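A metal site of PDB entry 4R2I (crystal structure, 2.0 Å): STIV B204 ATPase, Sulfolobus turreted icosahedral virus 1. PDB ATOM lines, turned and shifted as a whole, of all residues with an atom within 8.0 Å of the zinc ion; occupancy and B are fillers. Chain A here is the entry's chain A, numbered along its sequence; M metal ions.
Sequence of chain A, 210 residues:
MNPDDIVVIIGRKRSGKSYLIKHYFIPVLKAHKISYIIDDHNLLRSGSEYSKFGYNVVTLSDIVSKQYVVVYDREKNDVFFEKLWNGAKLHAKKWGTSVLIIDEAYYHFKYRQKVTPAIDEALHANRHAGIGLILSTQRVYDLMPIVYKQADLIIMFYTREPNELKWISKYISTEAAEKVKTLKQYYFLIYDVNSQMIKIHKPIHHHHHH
The side-chain carboxylate (OD1) of Asp 73 sits at hydrogen-bond distance from the backbone NH (N) of Glu 75, at 3.0 Å.
The backbone carbonyl oxygen (O) of Asp 39 is in hydrogen-bond range of the backbone NH (N) of Asp 103, 3.3 Å away.
The backbone carbonyl oxygen (O) of Asp 103 sits at hydrogen-bond distance from a ring nitrogen (ND1) of His 41 (2.8 Å).
The backbone NH (N) of Asp 39 is in hydrogen-bond range of the backbone carbonyl oxygen (O) of Ile 101, 2.8 Å away.
The backbone carbonyl oxygen (O) of Asp 40 sits at hydrogen-bond distance from the backbone NH (N) of Asp 73 (2.8 Å).
The side-chain carboxylate (OD1) of Asp 73 lies within hydrogen-bond range of the backbone NH (N) of Lys 76 (2.7 Å).
NE2 of His 108 is bound to the zinc ion.
A ring nitrogen (NE2) of His 41 binds the zinc ion, at 2.1 Å.
The zinc ion is bound by OD2 of Asp 73 (2.2 Å).
OD2 of Asp 39 binds the zinc ion (2.3 Å).
The side-chain carboxylate (OD1) of Asp 39 binds the zinc ion (2.4 Å).
The zinc ion has five donor atoms within binding distance.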
ATOM      1  N   ILE A  38      24.190 -20.368  -0.915  1.00  0.00           N
ATOM      2  CA  ILE A  38      22.849 -20.561  -0.442  1.00  0.00           C
ATOM      3  C   ILE A  38      22.204 -21.749  -1.196  1.00  0.00           C
ATOM      4  O   ILE A  38      22.056 -21.712  -2.407  1.00  0.00           O
ATOM      5  CB  ILE A  38      21.987 -19.313  -0.685  1.00  0.00           C
ATOM      6  CG1 ILE A  38      22.556 -18.132   0.101  1.00  0.00           C
ATOM      7  CG2 ILE A  38      20.554 -19.568  -0.229  1.00  0.00           C
ATOM      8  CD1 ILE A  38      22.167 -16.780  -0.461  1.00  0.00           C
ATOM      9  N   ASP A  39      21.863 -22.784  -0.424  1.00  0.00           N
ATOM     10  CA  ASP A  39      21.103 -23.946  -0.892  1.00  0.00           C
ATOM     11  C   ASP A  39      19.586 -23.637  -0.710  1.00  0.00           C
ATOM     12  O   ASP A  39      19.063 -23.609   0.394  1.00  0.00           O
ATOM     13  CB  ASP A  39      21.604 -25.181  -0.212  1.00  0.00           C
ATOM     14  CG  ASP A  39      20.765 -26.396  -0.480  1.00  0.00           C
ATOM     15  OD1 ASP A  39      20.315 -26.542  -1.606  1.00  0.00           O
ATOM     16  OD2 ASP A  39      20.600 -27.145   0.479  1.00  0.00           O
ATOM     17  N   ASP A  40      18.966 -23.275  -1.829  1.00  0.00           N
ATOM     18  CA  ASP A  40      17.595 -22.774  -1.870  1.00  0.00           C
ATOM     19  C   ASP A  40      16.736 -23.836  -2.584  1.00  0.00           C
ATOM     20  O   ASP A  40      17.101 -24.287  -3.693  1.00  0.00           O
ATOM     21  CB  ASP A  40      17.528 -21.451  -2.665  1.00  0.00           C
ATOM     22  CG  ASP A  40      16.142 -20.777  -2.591  1.00  0.00           C
ATOM     23  OD1 ASP A  40      15.181 -21.304  -1.944  1.00  0.00           O
ATOM     24  OD2 ASP A  40      16.011 -19.698  -3.182  1.00  0.00           O
ATOM     25  N   HIS A  41      15.656 -24.262  -1.910  1.00  0.00           N
ATOM     26  CA  HIS A  41      14.714 -25.306  -2.404  1.00  0.00           C
ATOM     27  C   HIS A  41      13.357 -24.759  -2.836  1.00  0.00           C
ATOM     28  O   HIS A  41      12.591 -25.454  -3.484  1.00  0.00           O
ATOM     29  CB  HIS A  41      14.446 -26.281  -1.276  1.00  0.00           C
ATOM     30  CG  HIS A  41      15.682 -26.804  -0.636  1.00  0.00           C
ATOM     31  ND1 HIS A  41      16.186 -26.297   0.542  1.00  0.00           N
ATOM     32  CD2 HIS A  41      16.571 -27.713  -1.061  1.00  0.00           C
ATOM     33  CE1 HIS A  41      17.296 -26.942   0.853  1.00  0.00           C
ATOM     34  NE2 HIS A  41      17.558 -27.794  -0.125  1.00  0.00           N
ATOM     35  N   VAL A  71      22.285 -21.557  -5.027  1.00  0.00           N
ATOM     36  CA  VAL A  71      22.055 -22.824  -5.721  1.00  0.00           C
ATOM     37  C   VAL A  71      20.562 -23.207  -5.667  1.00  0.00           C
ATOM     38  O   VAL A  71      20.005 -23.394  -4.588  1.00  0.00           O
ATOM     39  CB  VAL A  71      22.869 -23.995  -5.103  1.00  0.00           C
ATOM     40  CG1 VAL A  71      22.787 -25.210  -6.011  1.00  0.00           C
ATOM     41  CG2 VAL A  71      24.330 -23.623  -4.943  1.00  0.00           C
ATOM     42  N   TYR A  72      19.920 -23.393  -6.821  1.00  0.00           N
ATOM     43  CA  TYR A  72      18.563 -23.974  -6.841  1.00  0.00           C
ATOM     44  C   TYR A  72      18.633 -25.529  -6.692  1.00  0.00           C
ATOM     45  O   TYR A  72      19.266 -26.223  -7.499  1.00  0.00           O
ATOM     46  CB  TYR A  72      17.755 -23.476  -8.053  1.00  0.00           C
ATOM     47  CG  TYR A  72      17.897 -21.953  -8.242  1.00  0.00           C
ATOM     48  CD1 TYR A  72      17.525 -21.054  -7.232  1.00  0.00           C
ATOM     49  CD2 TYR A  72      18.466 -21.423  -9.408  1.00  0.00           C
ATOM     50  CE1 TYR A  72      17.703 -19.665  -7.382  1.00  0.00           C
ATOM     51  CE2 TYR A  72      18.637 -20.045  -9.577  1.00  0.00           C
ATOM     52  CZ  TYR A  72      18.269 -19.169  -8.559  1.00  0.00           C
ATOM     53  OH  TYR A  72      18.457 -17.804  -8.754  1.00  0.00           O
ATOM     54  N   ASP A  73      18.023 -26.067  -5.632  1.00  0.00           N
ATOM     55  CA  ASP A  73      18.025 -27.508  -5.407  1.00  0.00           C
ATOM     56  C   ASP A  73      16.602 -28.124  -5.567  1.00  0.00           C
ATOM     57  O   ASP A  73      15.807 -28.119  -4.624  1.00  0.00           O
ATOM     58  CB  ASP A  73      18.607 -27.830  -4.027  1.00  0.00           C
ATOM     59  CG  ASP A  73      18.679 -29.298  -3.740  1.00  0.00           C
ATOM     60  OD1 ASP A  73      18.461 -30.147  -4.634  1.00  0.00           O
ATOM     61  OD2 ASP A  73      18.981 -29.658  -2.601  1.00  0.00           O
ATOM     62  N   ARG A  74      16.277 -28.612  -6.754  1.00  0.00           N
ATOM     63  CA  ARG A  74      14.975 -29.325  -6.918  1.00  0.00           C
ATOM     64  C   ARG A  74      15.151 -30.836  -6.643  1.00  0.00           C
ATOM     65  O   ARG A  74      14.193 -31.544  -6.396  1.00  0.00           O
ATOM     66  CB  ARG A  74      14.245 -28.977  -8.228  1.00  0.00           C
ATOM     67  CG  ARG A  74      15.046 -29.127  -9.522  1.00  0.00           C
ATOM     68  CD  ARG A  74      14.969 -30.548 -10.062  1.00  0.00           C
ATOM     69  NE  ARG A  74      16.272 -31.033 -10.504  1.00  0.00           N
ATOM     70  CZ  ARG A  74      16.473 -32.136 -11.232  1.00  0.00           C
ATOM     71  NH1 ARG A  74      15.443 -32.905 -11.589  1.00  0.00           N
ATOM     72  NH2 ARG A  74      17.720 -32.474 -11.582  1.00  0.00           N
ATOM     73  N   GLU A  75      16.405 -31.272  -6.570  1.00  0.00           N
ATOM     74  CA  GLU A  75      16.799 -32.633  -6.158  1.00  0.00           C
ATOM     75  C   GLU A  75      16.447 -33.028  -4.699  1.00  0.00           C
ATOM     76  O   GLU A  75      15.762 -34.051  -4.457  1.00  0.00           O
ATOM     77  CB  GLU A  75      18.325 -32.759  -6.321  1.00  0.00           C
ATOM     78  CG  GLU A  75      18.817 -34.143  -6.646  1.00  0.00           C
ATOM     79  CD  GLU A  75      18.537 -34.508  -8.084  1.00  0.00           C
ATOM     80  OE1 GLU A  75      18.046 -33.626  -8.838  1.00  0.00           O
ATOM     81  OE2 GLU A  75      18.802 -35.685  -8.411  1.00  0.00           O
ATOM     82  N   LYS A  76      16.984 -32.250  -3.741  1.00  0.00           N
ATOM     83  CA  LYS A  76      16.622 -32.321  -2.317  1.00  0.00           C
ATOM     84  C   LYS A  76      17.048 -33.602  -1.637  1.00  0.00           C
ATOM     85  O   LYS A  76      16.371 -34.113  -0.743  1.00  0.00           O
ATOM     86  CB  LYS A  76      15.136 -32.041  -2.118  1.00  0.00           C
ATOM     87  CG  LYS A  76      14.750 -30.674  -2.677  1.00  0.00           C
ATOM     88  CD  LYS A  76      13.255 -30.430  -2.568  1.00  0.00           C
ATOM     89  CE  LYS A  76      12.833 -29.307  -3.509  1.00  0.00           C
ATOM     90  NZ  LYS A  76      11.485 -28.921  -3.085  1.00  0.00           N
ATOM     91  N   ASN A  77      18.283 -33.977  -1.973  1.00  0.00           N
ATOM     92  CA  ASN A  77      18.738 -35.350  -2.091  1.00  0.00           C
ATOM     93  C   ASN A  77      20.138 -35.522  -1.504  1.00  0.00           C
ATOM     94  O   ASN A  77      20.933 -34.577  -1.517  1.00  0.00           O
ATOM     95  CB  ASN A  77      18.859 -35.575  -3.614  1.00  0.00           C
ATOM     96  CG  ASN A  77      18.455 -36.934  -4.040  1.00  0.00           C
ATOM     97  OD1 ASN A  77      18.297 -37.830  -3.219  1.00  0.00           O
ATOM     98  ND2 ASN A  77      18.281 -37.119  -5.334  1.00  0.00           N
ATOM     99  N   PHE A  80      22.578 -34.853  -4.223  1.00  0.00           N
ATOM    100  CA  PHE A  80      22.780 -33.443  -4.400  1.00  0.00           C
ATOM    101  C   PHE A  80      23.643 -32.845  -3.274  1.00  0.00           C
ATOM    102  O   PHE A  80      24.478 -32.009  -3.532  1.00  0.00           O
ATOM    103  CB  PHE A  80      21.479 -32.713  -4.449  1.00  0.00           C
ATOM    104  CG  PHE A  80      21.635 -31.250  -4.744  1.00  0.00           C
ATOM    105  CD1 PHE A  80      21.695 -30.794  -6.069  1.00  0.00           C
ATOM    106  CD2 PHE A  80      21.777 -30.329  -3.713  1.00  0.00           C
ATOM    107  CE1 PHE A  80      21.864 -29.457  -6.349  1.00  0.00           C
ATOM    108  CE2 PHE A  80      21.946 -28.972  -3.982  1.00  0.00           C
ATOM    109  CZ  PHE A  80      21.979 -28.541  -5.305  1.00  0.00           C
ATOM    110  N   PHE A  81      23.422 -33.253  -2.018  1.00  0.00           N
ATOM    111  CA  PHE A  81      24.211 -32.699  -0.922  1.00  0.00           C
ATOM    112  C   PHE A  81      25.732 -32.993  -1.011  1.00  0.00           C
ATOM    113  O   PHE A  81      26.597 -32.139  -0.623  1.00  0.00           O
ATOM    114  CB  PHE A  81      23.714 -33.157   0.420  1.00  0.00           C
ATOM    115  CG  PHE A  81      24.365 -32.430   1.519  1.00  0.00           C
ATOM    116  CD1 PHE A  81      23.955 -31.149   1.826  1.00  0.00           C
ATOM    117  CD2 PHE A  81      25.478 -32.943   2.115  1.00  0.00           C
ATOM    118  CE1 PHE A  81      24.616 -30.403   2.780  1.00  0.00           C
ATOM    119  CE2 PHE A  81      26.161 -32.193   3.070  1.00  0.00           C
ATOM    120  CZ  PHE A  81      25.716 -30.915   3.386  1.00  0.00           C
ATOM    121  N   LEU A  84      26.947 -30.436  -3.481  1.00  0.00           N
ATOM    122  CA  LEU A  84      26.884 -29.102  -2.803  1.00  0.00           C
ATOM    123  C   LEU A  84      28.070 -28.975  -1.859  1.00  0.00           C
ATOM    124  O   LEU A  84      28.732 -27.933  -1.806  1.00  0.00           O
ATOM    125  CB  LEU A  84      25.608 -28.971  -1.984  1.00  0.00           C
ATOM    126  CG  LEU A  84      25.417 -27.685  -1.183  1.00  0.00           C
ATOM    127  CD1 LEU A  84      25.141 -26.493  -2.103  1.00  0.00           C
ATOM    128  CD2 LEU A  84      24.283 -27.909  -0.201  1.00  0.00           C
ATOM    129  N   ILE A 101      24.764 -21.791   3.554  1.00  0.00           N
ATOM    130  CA  ILE A 101      23.516 -21.404   4.127  1.00  0.00           C
ATOM    131  C   ILE A 101      22.447 -22.321   3.479  1.00  0.00           C
ATOM    132  O   ILE A 101      22.196 -22.292   2.282  1.00  0.00           O
ATOM    133  CB  ILE A 101      23.199 -19.946   3.858  1.00  0.00           C
ATOM    134  CG1 ILE A 101      24.325 -19.054   4.419  1.00  0.00           C
ATOM    135  CG2 ILE A 101      21.816 -19.570   4.442  1.00  0.00           C
ATOM    136  CD1 ILE A 101      24.198 -17.574   4.046  1.00  0.00           C
ATOM    137  N   ILE A 102      21.856 -23.134   4.324  1.00  0.00           N
ATOM    138  CA  ILE A 102      20.859 -24.089   3.917  1.00  0.00           C
ATOM    139  C   ILE A 102      19.479 -23.756   4.498  1.00  0.00           C
ATOM    140  O   ILE A 102      19.214 -23.922   5.678  1.00  0.00           O
ATOM    141  CB  ILE A 102      21.322 -25.502   4.319  1.00  0.00           C
ATOM    142  CG1 ILE A 102      22.653 -25.785   3.596  1.00  0.00           C
ATOM    143  CG2 ILE A 102      20.241 -26.530   3.958  1.00  0.00           C
ATOM    144  CD1 ILE A 102      23.347 -27.013   4.030  1.00  0.00           C
ATOM    145  N   ASP A 103      18.611 -23.298   3.623  1.00  0.00           N
ATOM    146  CA  ASP A 103      17.254 -22.983   4.000  1.00  0.00           C
ATOM    147  C   ASP A 103      16.506 -24.305   3.876  1.00  0.00           C
ATOM    148  O   ASP A 103      16.795 -25.093   2.981  1.00  0.00           O
ATOM    149  CB  ASP A 103      16.759 -21.929   3.011  1.00  0.00           C
ATOM    150  CG  ASP A 103      15.368 -21.435   3.339  1.00  0.00           C
ATOM    151  OD1 ASP A 103      15.158 -20.911   4.479  1.00  0.00           O
ATOM    152  OD2 ASP A 103      14.503 -21.589   2.448  1.00  0.00           O
ATOM    153  N   GLU A 104      15.590 -24.567   4.797  1.00  0.00           N
ATOM    154  CA  GLU A 104      14.866 -25.814   4.929  1.00  0.00           C
ATOM    155  C   GLU A 104      15.858 -26.955   4.950  1.00  0.00           C
ATOM    156  O   GLU A 104      15.860 -27.787   4.054  1.00  0.00           O
ATOM    157  CB  GLU A 104      13.836 -25.966   3.798  1.00  0.00           C
ATOM    158  CG  GLU A 104      12.859 -24.810   3.806  1.00  0.00           C
ATOM    159  CD  GLU A 104      11.841 -24.914   2.729  1.00  0.00           C
ATOM    160  OE1 GLU A 104      12.206 -24.747   1.540  1.00  0.00           O
ATOM    161  OE2 GLU A 104      10.667 -25.179   3.081  1.00  0.00           O
ATOM    162  N   ALA A 105      16.677 -26.952   5.985  1.00  0.00           N
ATOM    163  CA  ALA A 105      17.759 -27.877   6.118  1.00  0.00           C
ATOM    164  C   ALA A 105      17.248 -29.277   6.389  1.00  0.00           C
ATOM    165  O   ALA A 105      17.998 -30.214   6.198  1.00  0.00           O
ATOM    166  CB  ALA A 105      18.702 -27.448   7.228  1.00  0.00           C
ATOM    167  N   TYR A 106      15.971 -29.391   6.756  1.00  0.00           N
ATOM    168  CA  TYR A 106      15.215 -30.663   6.746  1.00  0.00           C
ATOM    169  C   TYR A 106      15.588 -31.568   5.570  1.00  0.00           C
ATOM    170  O   TYR A 106      15.781 -32.760   5.728  1.00  0.00           O
ATOM    171  CB  TYR A 106      13.705 -30.329   6.700  1.00  0.00           C
ATOM    172  CG  TYR A 106      12.840 -31.479   6.360  1.00  0.00           C
ATOM    173  CD1 TYR A 106      12.577 -32.482   7.330  1.00  0.00           C
ATOM    174  CD2 TYR A 106      12.284 -31.616   5.077  1.00  0.00           C
ATOM    175  CE1 TYR A 106      11.776 -33.588   7.017  1.00  0.00           C
ATOM    176  CE2 TYR A 106      11.483 -32.722   4.764  1.00  0.00           C
ATOM    177  CZ  TYR A 106      11.229 -33.696   5.724  1.00  0.00           C
ATOM    178  OH  TYR A 106      10.452 -34.784   5.414  1.00  0.00           O
ATOM    179  N   TYR A 107      15.686 -31.014   4.380  1.00  0.00           N
ATOM    180  CA  TYR A 107      15.880 -31.825   3.185  1.00  0.00           C
ATOM    181  C   TYR A 107      17.134 -32.681   3.266  1.00  0.00           C
ATOM    182  O   TYR A 107      17.149 -33.835   2.836  1.00  0.00           O
ATOM    183  CB  TYR A 107      15.872 -30.940   1.965  1.00  0.00           C
ATOM    184  CG  TYR A 107      14.503 -30.418   1.617  1.00  0.00           C
ATOM    185  CD1 TYR A 107      13.484 -31.299   1.223  1.00  0.00           C
ATOM    186  CD2 TYR A 107      14.227 -29.030   1.597  1.00  0.00           C
ATOM    187  CE1 TYR A 107      12.214 -30.820   0.876  1.00  0.00           C
ATOM    188  CE2 TYR A 107      12.967 -28.564   1.275  1.00  0.00           C
ATOM    189  CZ  TYR A 107      11.979 -29.474   0.898  1.00  0.00           C
ATOM    190  OH  TYR A 107      10.745 -29.043   0.544  1.00  0.00           O
ATOM    191  N   HIS A 108      18.185 -32.156   3.895  1.00  0.00           N
ATOM    192  CA  HIS A 108      19.418 -32.899   4.009  1.00  0.00           C
ATOM    193  C   HIS A 108      19.822 -33.300   5.423  1.00  0.00           C
ATOM    194  O   HIS A 108      20.724 -34.135   5.568  1.00  0.00           O
ATOM    195  CB  HIS A 108      20.583 -32.121   3.413  1.00  0.00           C
ATOM    196  CG  HIS A 108      20.280 -31.455   2.111  1.00  0.00           C
ATOM    197  ND1 HIS A 108      20.068 -32.158   0.938  1.00  0.00           N
ATOM    198  CD2 HIS A 108      20.236 -30.144   1.776  1.00  0.00           C
ATOM    199  CE1 HIS A 108      19.857 -31.298  -0.049  1.00  0.00           C
ATOM    200  NE2 HIS A 108      19.959 -30.068   0.430  1.00  0.00           N
ATOM    201  N   PHE A 109      19.213 -32.686   6.458  1.00  0.00           N
ATOM    202  CA  PHE A 109      19.643 -32.944   7.850  1.00  0.00           C
ATOM    203  C   PHE A 109      18.589 -33.631   8.706  1.00  0.00           C
ATOM    204  O   PHE A 109      18.696 -33.669   9.910  1.00  0.00           O
ATOM    205  CB  PHE A 109      20.102 -31.632   8.495  1.00  0.00           C
ATOM    206  CG  PHE A 109      21.429 -31.139   7.954  1.00  0.00           C
ATOM    207  CD1 PHE A 109      21.482 -30.361   6.806  1.00  0.00           C
ATOM    208  CD2 PHE A 109      22.627 -31.578   8.504  1.00  0.00           C
ATOM    209  CE1 PHE A 109      22.697 -29.962   6.284  1.00  0.00           C
ATOM    210  CE2 PHE A 109      23.842 -31.180   7.982  1.00  0.00           C
ATOM    211  CZ  PHE A 109      23.894 -30.379   6.881  1.00  0.00           C
HETATM  212 ZN    ZN M   1      19.360 -28.586  -0.761  1.00  0.00          ZN
